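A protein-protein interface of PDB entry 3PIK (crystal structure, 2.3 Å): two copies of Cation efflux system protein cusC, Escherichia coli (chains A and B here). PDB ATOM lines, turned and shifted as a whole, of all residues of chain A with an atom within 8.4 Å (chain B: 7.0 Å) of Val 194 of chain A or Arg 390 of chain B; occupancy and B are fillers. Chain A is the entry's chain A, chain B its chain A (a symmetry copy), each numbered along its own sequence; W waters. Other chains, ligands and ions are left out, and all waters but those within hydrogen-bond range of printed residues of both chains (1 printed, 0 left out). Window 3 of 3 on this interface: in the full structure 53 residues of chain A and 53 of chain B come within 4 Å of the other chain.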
ATOM      1  N   TYR A 180       6.143  -6.335 -32.266  1.00  0.00           N
ATOM      2  CA  TYR A 180       6.996  -7.294 -31.586  1.00  0.00           C
ATOM      3  C   TYR A 180       8.477  -6.910 -31.698  1.00  0.00           C
ATOM      4  O   TYR A 180       9.208  -6.942 -30.708  1.00  0.00           O
ATOM      5  CB  TYR A 180       6.749  -8.700 -32.143  1.00  0.00           C
ATOM      6  CG  TYR A 180       7.650  -9.760 -31.549  1.00  0.00           C
ATOM      7  CD1 TYR A 180       7.331 -10.383 -30.346  1.00  0.00           C
ATOM      8  CD2 TYR A 180       8.816 -10.152 -32.201  1.00  0.00           C
ATOM      9  CE1 TYR A 180       8.149 -11.362 -29.808  1.00  0.00           C
ATOM     10  CE2 TYR A 180       9.641 -11.127 -31.670  1.00  0.00           C
ATOM     11  CZ  TYR A 180       9.307 -11.724 -30.472  1.00  0.00           C
ATOM     12  OH  TYR A 180      10.126 -12.691 -29.948  1.00  0.00           O
ATOM     13  N   VAL A 183       9.217  -4.268 -29.230  1.00  0.00           N
ATOM     14  CA  VAL A 183       9.288  -4.657 -27.824  1.00  0.00           C
ATOM     15  C   VAL A 183      10.612  -5.390 -27.548  1.00  0.00           C
ATOM     16  O   VAL A 183      11.223  -5.232 -26.496  1.00  0.00           O
ATOM     17  CB  VAL A 183       8.075  -5.505 -27.384  1.00  0.00           C
ATOM     18  CG1 VAL A 183       8.309  -6.055 -25.983  1.00  0.00           C
ATOM     19  CG2 VAL A 183       6.764  -4.669 -27.445  1.00  0.00           C
ATOM     20  N   LEU A 187      13.516  -4.537 -24.860  1.00  0.00           N
ATOM     21  CA  LEU A 187      14.029  -5.510 -23.924  1.00  0.00           C
ATOM     22  C   LEU A 187      15.552  -5.546 -24.002  1.00  0.00           C
ATOM     23  O   LEU A 187      16.230  -5.718 -22.991  1.00  0.00           O
ATOM     24  CB  LEU A 187      13.444  -6.888 -24.236  1.00  0.00           C
ATOM     25  CG  LEU A 187      13.258  -7.799 -23.026  1.00  0.00           C
ATOM     26  CD1 LEU A 187      12.399  -7.111 -21.983  1.00  0.00           C
ATOM     27  CD2 LEU A 187      12.640  -9.120 -23.445  1.00  0.00           C
ATOM     28  N   SER A 191      14.427  -2.285 -20.977  1.00  0.00           N
ATOM     29  CA  SER A 191      13.451  -1.208 -20.860  1.00  0.00           C
ATOM     30  C   SER A 191      12.009  -1.692 -20.774  1.00  0.00           C
ATOM     31  O   SER A 191      11.129  -0.968 -20.296  1.00  0.00           O
ATOM     32  CB  SER A 191      13.585  -0.245 -22.029  1.00  0.00           C
ATOM     33  OG  SER A 191      12.318   0.295 -22.356  1.00  0.00           O
ATOM     34  N   SER A 192      11.751  -2.900 -21.255  1.00  0.00           N
ATOM     35  CA  SER A 192      10.415  -3.464 -21.119  1.00  0.00           C
ATOM     36  C   SER A 192      10.485  -4.721 -20.275  1.00  0.00           C
ATOM     37  O   SER A 192      11.394  -4.887 -19.465  1.00  0.00           O
ATOM     38  CB  SER A 192       9.812  -3.797 -22.488  1.00  0.00           C
ATOM     39  OG  SER A 192       8.442  -4.113 -22.349  1.00  0.00           O
ATOM     40  N   ASN A 193       9.528  -5.615 -20.469  1.00  0.00           N
ATOM     41  CA  ASN A 193       9.564  -6.884 -19.767  1.00  0.00           C
ATOM     42  C   ASN A 193       9.128  -8.074 -20.612  1.00  0.00           C
ATOM     43  O   ASN A 193       8.662  -7.938 -21.749  1.00  0.00           O
ATOM     44  CB  ASN A 193       8.793  -6.830 -18.442  1.00  0.00           C
ATOM     45  CG  ASN A 193       7.309  -6.660 -18.644  1.00  0.00           C
ATOM     46  OD1 ASN A 193       6.657  -7.503 -19.266  1.00  0.00           O
ATOM     47  ND2 ASN A 193       6.754  -5.576 -18.105  1.00  0.00           N
ATOM     48  N   VAL A 194       9.294  -9.248 -20.030  1.00  0.00           N
ATOM     49  CA  VAL A 194       9.173 -10.479 -20.766  1.00  0.00           C
ATOM     50  C   VAL A 194       7.692 -10.795 -20.961  1.00  0.00           C
ATOM     51  O   VAL A 194       7.328 -11.571 -21.826  1.00  0.00           O
ATOM     52  CB  VAL A 194       9.959 -11.611 -20.040  1.00  0.00           C
ATOM     53  CG1 VAL A 194       9.311 -11.963 -18.704  1.00  0.00           C
ATOM     54  CG2 VAL A 194      10.106 -12.828 -20.921  1.00  0.00           C
ATOM     55  N   LEU A 195       6.839 -10.157 -20.165  1.00  0.00           N
ATOM     56  CA  LEU A 195       5.405 -10.328 -20.302  1.00  0.00           C
ATOM     57  C   LEU A 195       4.929  -9.640 -21.576  1.00  0.00           C
ATOM     58  O   LEU A 195       4.258 -10.253 -22.404  1.00  0.00           O
ATOM     59  CB  LEU A 195       4.655  -9.777 -19.088  1.00  0.00           C
ATOM     60  CG  LEU A 195       3.128  -9.708 -19.248  1.00  0.00           C
ATOM     61  CD1 LEU A 195       2.545 -11.117 -19.486  1.00  0.00           C
ATOM     62  CD2 LEU A 195       2.461  -9.037 -18.045  1.00  0.00           C
ATOM     63  N   ALA A 196       5.290  -8.367 -21.726  1.00  0.00           N
ATOM     64  CA  ALA A 196       4.925  -7.586 -22.902  1.00  0.00           C
ATOM     65  C   ALA A 196       5.396  -8.291 -24.170  1.00  0.00           C
ATOM     66  O   ALA A 196       4.690  -8.315 -25.173  1.00  0.00           O
ATOM     67  CB  ALA A 196       5.535  -6.198 -22.819  1.00  0.00           C
ATOM     68  N   LEU A 197       6.597  -8.866 -24.119  1.00  0.00           N
ATOM     69  CA  LEU A 197       7.158  -9.550 -25.273  1.00  0.00           C
ATOM     70  C   LEU A 197       6.315 -10.767 -25.664  1.00  0.00           C
ATOM     71  O   LEU A 197       6.016 -10.986 -26.832  1.00  0.00           O
ATOM     72  CB  LEU A 197       8.590 -10.003 -24.989  1.00  0.00           C
ATOM     73  CG  LEU A 197       9.277 -10.604 -26.217  1.00  0.00           C
ATOM     74  CD1 LEU A 197       9.717  -9.492 -27.153  1.00  0.00           C
ATOM     75  CD2 LEU A 197      10.457 -11.478 -25.829  1.00  0.00           C
ATOM     76  N   GLU A 198       5.945 -11.575 -24.681  1.00  0.00           N
ATOM     77  CA  GLU A 198       5.161 -12.750 -24.986  1.00  0.00           C
ATOM     78  C   GLU A 198       3.768 -12.347 -25.504  1.00  0.00           C
ATOM     79  O   GLU A 198       3.201 -13.007 -26.371  1.00  0.00           O
ATOM     80  CB  GLU A 198       5.045 -13.656 -23.767  1.00  0.00           C
ATOM     81  CG  GLU A 198       4.717 -15.093 -24.138  1.00  0.00           C
ATOM     82  CD  GLU A 198       5.783 -15.681 -25.043  1.00  0.00           C
ATOM     83  OE1 GLU A 198       6.973 -15.348 -24.850  1.00  0.00           O
ATOM     84  OE2 GLU A 198       5.438 -16.442 -25.960  1.00  0.00           O
ATOM     85  N   GLN A 199       3.219 -11.261 -24.968  1.00  0.00           N
ATOM     86  CA  GLN A 199       1.945 -10.767 -25.457  1.00  0.00           C
ATOM     87  C   GLN A 199       2.039 -10.370 -26.930  1.00  0.00           C
ATOM     88  O   GLN A 199       1.173 -10.734 -27.723  1.00  0.00           O
ATOM     89  CB  GLN A 199       1.448  -9.610 -24.596  1.00  0.00           C
ATOM     90  CG  GLN A 199       1.025 -10.055 -23.198  1.00  0.00           C
ATOM     91  CD  GLN A 199       0.783  -8.894 -22.272  1.00  0.00           C
ATOM     92  OE1 GLN A 199       1.492  -7.890 -22.321  1.00  0.00           O
ATOM     93  NE2 GLN A 199      -0.213  -9.026 -21.407  1.00  0.00           N
ATOM     94  N   ALA A 200       3.101  -9.657 -27.301  1.00  0.00           N
ATOM     95  CA  ALA A 200       3.273  -9.248 -28.689  1.00  0.00           C
ATOM     96  C   ALA A 200       3.482 -10.453 -29.594  1.00  0.00           C
ATOM     97  O   ALA A 200       3.080 -10.439 -30.760  1.00  0.00           O
ATOM     98  CB  ALA A 200       4.424  -8.276 -28.832  1.00  0.00           C
ATOM     99  N   ARG A 201       4.110 -11.495 -29.061  1.00  0.00           N
ATOM    100  CA  ARG A 201       4.344 -12.690 -29.860  1.00  0.00           C
ATOM    101  C   ARG A 201       3.039 -13.441 -30.110  1.00  0.00           C
ATOM    102  O   ARG A 201       2.744 -13.859 -31.239  1.00  0.00           O
ATOM    103  CB  ARG A 201       5.357 -13.612 -29.190  1.00  0.00           C
ATOM    104  CG  ARG A 201       5.542 -14.934 -29.922  1.00  0.00           C
ATOM    105  CD  ARG A 201       7.000 -15.187 -30.204  1.00  0.00           C
ATOM    106  NE  ARG A 201       7.345 -16.600 -30.108  1.00  0.00           N
ATOM    107  CZ  ARG A 201       8.585 -17.068 -30.193  1.00  0.00           C
ATOM    108  NH1 ARG A 201       9.601 -16.234 -30.379  1.00  0.00           N
ATOM    109  NH2 ARG A 201       8.812 -18.370 -30.089  1.00  0.00           N
ATOM    110  N   TYR A 395       2.506   3.746 -22.912  1.00  0.00           N
ATOM    111  CA  TYR A 395       3.254   2.541 -22.598  1.00  0.00           C
ATOM    112  C   TYR A 395       4.751   2.773 -22.747  1.00  0.00           C
ATOM    113  O   TYR A 395       5.544   2.344 -21.909  1.00  0.00           O
ATOM    114  CB  TYR A 395       2.832   1.371 -23.481  1.00  0.00           C
ATOM    115  CG  TYR A 395       3.864   0.268 -23.510  1.00  0.00           C
ATOM    116  CD1 TYR A 395       4.028  -0.598 -22.425  1.00  0.00           C
ATOM    117  CD2 TYR A 395       4.688   0.104 -24.613  1.00  0.00           C
ATOM    118  CE1 TYR A 395       4.985  -1.610 -22.454  1.00  0.00           C
ATOM    119  CE2 TYR A 395       5.651  -0.892 -24.646  1.00  0.00           C
ATOM    120  CZ  TYR A 395       5.796  -1.741 -23.571  1.00  0.00           C
ATOM    121  OH  TYR A 395       6.753  -2.726 -23.634  1.00  0.00           O
ATOM    122  N   LEU B 384       0.379 -18.326 -24.876  1.00  0.00           N
ATOM    123  CA  LEU B 384      -0.521 -17.903 -23.812  1.00  0.00           C
ATOM    124  C   LEU B 384      -0.164 -18.545 -22.461  1.00  0.00           C
ATOM    125  O   LEU B 384      -0.292 -17.917 -21.410  1.00  0.00           O
ATOM    126  CB  LEU B 384      -1.973 -18.174 -24.204  1.00  0.00           C
ATOM    127  CG  LEU B 384      -2.527 -17.246 -25.298  1.00  0.00           C
ATOM    128  CD1 LEU B 384      -3.871 -17.766 -25.843  1.00  0.00           C
ATOM    129  CD2 LEU B 384      -2.673 -15.802 -24.795  1.00  0.00           C
ATOM    130  N   GLN B 385       0.280 -19.799 -22.493  1.00  0.00           N
ATOM    131  CA  GLN B 385       0.704 -20.481 -21.279  1.00  0.00           C
ATOM    132  C   GLN B 385       1.875 -19.723 -20.643  1.00  0.00           C
ATOM    133  O   GLN B 385       1.897 -19.517 -19.426  1.00  0.00           O
ATOM    134  CB  GLN B 385       1.090 -21.943 -21.564  1.00  0.00           C
ATOM    135  CG  GLN B 385      -0.076 -22.815 -22.046  1.00  0.00           C
ATOM    136  CD  GLN B 385       0.348 -24.239 -22.420  1.00  0.00           C
ATOM    137  OE1 GLN B 385       1.462 -24.475 -22.885  1.00  0.00           O
ATOM    138  NE2 GLN B 385      -0.547 -25.190 -22.208  1.00  0.00           N
ATOM    139  N   ILE B 386       2.830 -19.303 -21.473  1.00  0.00           N
ATOM    140  CA  ILE B 386       3.982 -18.538 -20.996  1.00  0.00           C
ATOM    141  C   ILE B 386       3.539 -17.182 -20.432  1.00  0.00           C
ATOM    142  O   ILE B 386       3.936 -16.799 -19.335  1.00  0.00           O
ATOM    143  CB  ILE B 386       5.021 -18.325 -22.104  1.00  0.00           C
ATOM    144  CG1 ILE B 386       5.565 -19.673 -22.591  1.00  0.00           C
ATOM    145  CG2 ILE B 386       6.152 -17.423 -21.608  1.00  0.00           C
ATOM    146  CD1 ILE B 386       6.451 -19.555 -23.833  1.00  0.00           C
ATOM    147  N   THR B 387       2.701 -16.484 -21.192  1.00  0.00           N
ATOM    148  CA  THR B 387       2.098 -15.225 -20.779  1.00  0.00           C
ATOM    149  C   THR B 387       1.422 -15.336 -19.411  1.00  0.00           C
ATOM    150  O   THR B 387       1.617 -14.482 -18.545  1.00  0.00           O
ATOM    151  CB  THR B 387       1.037 -14.783 -21.811  1.00  0.00           C
ATOM    152  OG1 THR B 387       1.674 -14.543 -23.068  1.00  0.00           O
ATOM    153  CG2 THR B 387       0.308 -13.525 -21.363  1.00  0.00           C
ATOM    154  N   LEU B 388       0.620 -16.381 -19.218  1.00  0.00           N
ATOM    155  CA  LEU B 388      -0.044 -16.586 -17.925  1.00  0.00           C
ATOM    156  C   LEU B 388       0.979 -16.665 -16.794  1.00  0.00           C
ATOM    157  O   LEU B 388       0.855 -15.970 -15.786  1.00  0.00           O
ATOM    158  CB  LEU B 388      -0.886 -17.866 -17.943  1.00  0.00           C
ATOM    159  CG  LEU B 388      -1.716 -18.178 -16.694  1.00  0.00           C
ATOM    160  CD1 LEU B 388      -2.477 -16.942 -16.204  1.00  0.00           C
ATOM    161  CD2 LEU B 388      -2.682 -19.354 -16.937  1.00  0.00           C
ATOM    162  N   GLN B 389       1.980 -17.526 -16.972  1.00  0.00           N
ATOM    163  CA  GLN B 389       3.052 -17.688 -15.991  1.00  0.00           C
ATOM    164  C   GLN B 389       3.767 -16.363 -15.664  1.00  0.00           C
ATOM    165  O   GLN B 389       3.964 -16.032 -14.496  1.00  0.00           O
ATOM    166  CB  GLN B 389       4.053 -18.756 -16.445  1.00  0.00           C
ATOM    167  CG  GLN B 389       3.476 -20.173 -16.479  1.00  0.00           C
ATOM    168  CD  GLN B 389       2.841 -20.577 -15.150  1.00  0.00           C
ATOM    169  OE1 GLN B 389       3.382 -20.302 -14.072  1.00  0.00           O
ATOM    170  NE2 GLN B 389       1.677 -21.213 -15.221  1.00  0.00           N
ATOM    171  N   ARG B 390       4.133 -15.606 -16.688  1.00  0.00           N
ATOM    172  CA  ARG B 390       4.770 -14.300 -16.486  1.00  0.00           C
ATOM    173  C   ARG B 390       3.838 -13.327 -15.768  1.00  0.00           C
ATOM    174  O   ARG B 390       4.275 -12.559 -14.918  1.00  0.00           O
ATOM    175  CB  ARG B 390       5.188 -13.702 -17.828  1.00  0.00           C
ATOM    176  CG  ARG B 390       6.191 -14.544 -18.600  1.00  0.00           C
ATOM    177  CD  ARG B 390       7.419 -14.846 -17.742  1.00  0.00           C
ATOM    178  NE  ARG B 390       8.517 -15.384 -18.543  1.00  0.00           N
ATOM    179  CZ  ARG B 390       9.674 -15.811 -18.043  1.00  0.00           C
ATOM    180  NH1 ARG B 390       9.900 -15.780 -16.731  1.00  0.00           N
ATOM    181  NH2 ARG B 390      10.606 -16.276 -18.862  1.00  0.00           N
ATOM    182  N   ALA B 391       2.552 -13.350 -16.114  1.00  0.00           N
ATOM    183  CA  ALA B 391       1.604 -12.422 -15.496  1.00  0.00           C
ATOM    184  C   ALA B 391       1.445 -12.723 -14.012  1.00  0.00           C
ATOM    185  O   ALA B 391       1.361 -11.813 -13.191  1.00  0.00           O
ATOM    186  CB  ALA B 391       0.249 -12.466 -16.194  1.00  0.00           C
ATOM    187  N   ARG B 392       1.405 -14.005 -13.673  1.00  0.00           N
ATOM    188  CA  ARG B 392       1.278 -14.402 -12.274  1.00  0.00           C
ATOM    189  C   ARG B 392       2.456 -13.892 -11.465  1.00  0.00           C
ATOM    190  O   ARG B 392       2.279 -13.298 -10.405  1.00  0.00           O
ATOM    191  CB  ARG B 392       1.186 -15.921 -12.125  1.00  0.00           C
ATOM    192  CG  ARG B 392      -0.133 -16.524 -12.563  1.00  0.00           C
ATOM    193  CD  ARG B 392      -0.265 -17.949 -12.023  1.00  0.00           C
ATOM    194  NE  ARG B 392      -1.299 -18.740 -12.694  1.00  0.00           N
ATOM    195  CZ  ARG B 392      -2.600 -18.609 -12.474  1.00  0.00           C
ATOM    196  NH1 ARG B 392      -3.039 -17.694 -11.616  1.00  0.00           N
ATOM    197  NH2 ARG B 392      -3.463 -19.386 -13.119  1.00  0.00           N
ATOM    198  N   ALA B 393       3.659 -14.135 -11.974  1.00  0.00           N
ATOM    199  CA  ALA B 393       4.861 -13.731 -11.282  1.00  0.00           C
ATOM    200  C   ALA B 393       4.851 -12.215 -11.059  1.00  0.00           C
ATOM    201  O   ALA B 393       5.052 -11.744  -9.940  1.00  0.00           O
ATOM    202  CB  ALA B 393       6.099 -14.172 -12.055  1.00  0.00           C
ATOM    203  N   LEU B 394       4.602 -11.463 -12.124  1.00  0.00           N
ATOM    204  CA  LEU B 394       4.568 -10.003 -12.046  1.00  0.00           C
ATOM    205  C   LEU B 394       3.450  -9.509 -11.124  1.00  0.00           C
ATOM    206  O   LEU B 394       3.610  -8.525 -10.415  1.00  0.00           O
ATOM    207  CB  LEU B 394       4.375  -9.405 -13.435  1.00  0.00           C
ATOM    208  CG  LEU B 394       5.543  -8.773 -14.188  1.00  0.00           C
ATOM    209  CD1 LEU B 394       6.898  -9.183 -13.646  1.00  0.00           C
ATOM    210  CD2 LEU B 394       5.431  -9.078 -15.669  1.00  0.00           C
ATOM    211  N   TYR B 395       2.313 -10.191 -11.132  1.00  0.00           N
ATOM    212  CA  TYR B 395       1.214  -9.777 -10.277  1.00  0.00           C
ATOM    213  C   TYR B 395       1.534 -10.039  -8.812  1.00  0.00           C
ATOM    214  O   TYR B 395       1.272  -9.203  -7.948  1.00  0.00           O
ATOM    215  CB  TYR B 395      -0.085 -10.486 -10.648  1.00  0.00           C
ATOM    216  CG  TYR B 395      -1.105 -10.440  -9.534  1.00  0.00           C
ATOM    217  CD1 TYR B 395      -1.814  -9.271  -9.249  1.00  0.00           C
ATOM    218  CD2 TYR B 395      -1.346 -11.561  -8.754  1.00  0.00           C
ATOM    219  CE1 TYR B 395      -2.750  -9.232  -8.217  1.00  0.00           C
ATOM    220  CE2 TYR B 395      -2.266 -11.530  -7.717  1.00  0.00           C
ATOM    221  CZ  TYR B 395      -2.960 -10.369  -7.454  1.00  0.00           C
ATOM    222  OH  TYR B 395      -3.873 -10.368  -6.426  1.00  0.00           O
ATOM    223  N   GLN B 396       2.085 -11.215  -8.540  1.00  0.00           N
ATOM    224  CA  GLN B 396       2.403 -11.599  -7.174  1.00  0.00           C
ATOM    225  C   GLN B 396       3.523 -10.751  -6.582  1.00  0.00           C
ATOM    226  O   GLN B 396       3.733 -10.761  -5.376  1.00  0.00           O
ATOM    227  CB  GLN B 396       2.739 -13.090  -7.102  1.00  0.00           C
ATOM    228  CG  GLN B 396       1.565 -13.971  -7.561  1.00  0.00           C
ATOM    229  CD  GLN B 396       1.909 -15.447  -7.644  1.00  0.00           C
ATOM    230  OE1 GLN B 396       3.009 -15.864  -7.266  1.00  0.00           O
ATOM    231  NE2 GLN B 396       0.967 -16.249  -8.142  1.00  0.00           N
ATOM    232  N   VAL B 400       2.060  -5.574 -11.554  1.00  0.00           N
ATOM    233  CA  VAL B 400       0.930  -5.364 -12.468  1.00  0.00           C
ATOM    234  C   VAL B 400      -0.375  -5.768 -11.804  1.00  0.00           C
ATOM    235  O   VAL B 400      -0.386  -6.515 -10.823  1.00  0.00           O
ATOM    236  CB  VAL B 400       1.059  -6.178 -13.767  1.00  0.00           C
ATOM    237  CG1 VAL B 400       2.265  -5.731 -14.576  1.00  0.00           C
ATOM    238  CG2 VAL B 400       1.102  -7.684 -13.460  1.00  0.00           C
ATOM    239  N   VAL B 405      -3.651 -11.234 -15.148  1.00  0.00           N
ATOM    240  CA  VAL B 405      -3.843 -12.667 -14.914  1.00  0.00           C
ATOM    241  C   VAL B 405      -5.175 -13.118 -15.503  1.00  0.00           C
ATOM    242  O   VAL B 405      -5.253 -14.103 -16.247  1.00  0.00           O
ATOM    243  CB  VAL B 405      -3.762 -13.025 -13.409  1.00  0.00           C
ATOM    244  CG1 VAL B 405      -4.125 -14.492 -13.188  1.00  0.00           C
ATOM    245  CG2 VAL B 405      -2.368 -12.739 -12.857  1.00  0.00           C
HETATM  246  O   HOH W   1       0.382 -14.463 -25.449  1.00  0.00           O
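OD1 of Asn 193 of chain A is in hydrogen-bond range of N of Leu 195 of chain A (2.8 Å).
NE of Arg 390 of chain B touches CG1 of Val 194 of chain A, 3.5 Å away. Leu 195 of chain A touches Thr 387 of chain B (CD1 to O, 3.6 Å). Leu 394 of chain B touches Leu 195 of chain A. Glu 198 of chain A touches Ile 386 of chain B (CG to CG2, 3.7 Å). Glu 198 of chain A touches Thr 387 of chain B (CG to OG1, 3.3 Å). CG of Gln 199 of chain A touches CG2 of Thr 387 of chain B, 3.99 Å away.
Tyr 180 of chain A touches none of the printed residues of chain B. Of chain B, only Arg 390 comes within 4 Å of Val 194 of chain A. Of the printed residues of chain B, Leu 195 of chain A touches Thr 387 (3.6 Å) and Leu 394 (3.6 Å). Gln 385 of chain B touches none of the printed residues of chain A. Printed residues of chain A within 4 Å of Thr 387 of chain B: Leu 195, Glu 198 and Gln 199. Arg 390 of chain B touches just one residue of chain A: Val 194. Of the printed residues of chain A, Leu 394 of chain B touches Leu 195 (3.6 Å). The nearest residue of chain A that does not touch Arg 390 of chain B is Leu 195 of chain A (4.1 Å). The nearest printed residue of chain A that does not touch Leu 394 of chain B is Asn 193 of chain A (4.1 Å).
Of the 15 printed residues of chain A, 4 touch a printed residue of chain B. Printed residues of chain A that touch a printed residue of chain B: Val 194, Leu 195, Glu 198 and Gln 199. Hydrophobic or aromatic side chains of chain A within 4 Å of the printed part of chain B: Val 194 and Leu 195. Hydrophobic or aromatic side chains of chain B that line the printed part of chain A: Ile 386 and Leu 394. Among the printed residues, no Asp or Glu carboxylate lies within 4 Å of a Lys or Arg side-chain nitrogen of the other chain.
1 position is printed for both chains. Of the 6 pairs that touch across the chains among the printed residues, none has its exchanged pair printed and touching as well.
Water W1 bridges the side-chain hydroxyl of Thr 387 of chain B and the backbone carbonyl oxygen of Glu 198 of chain A.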
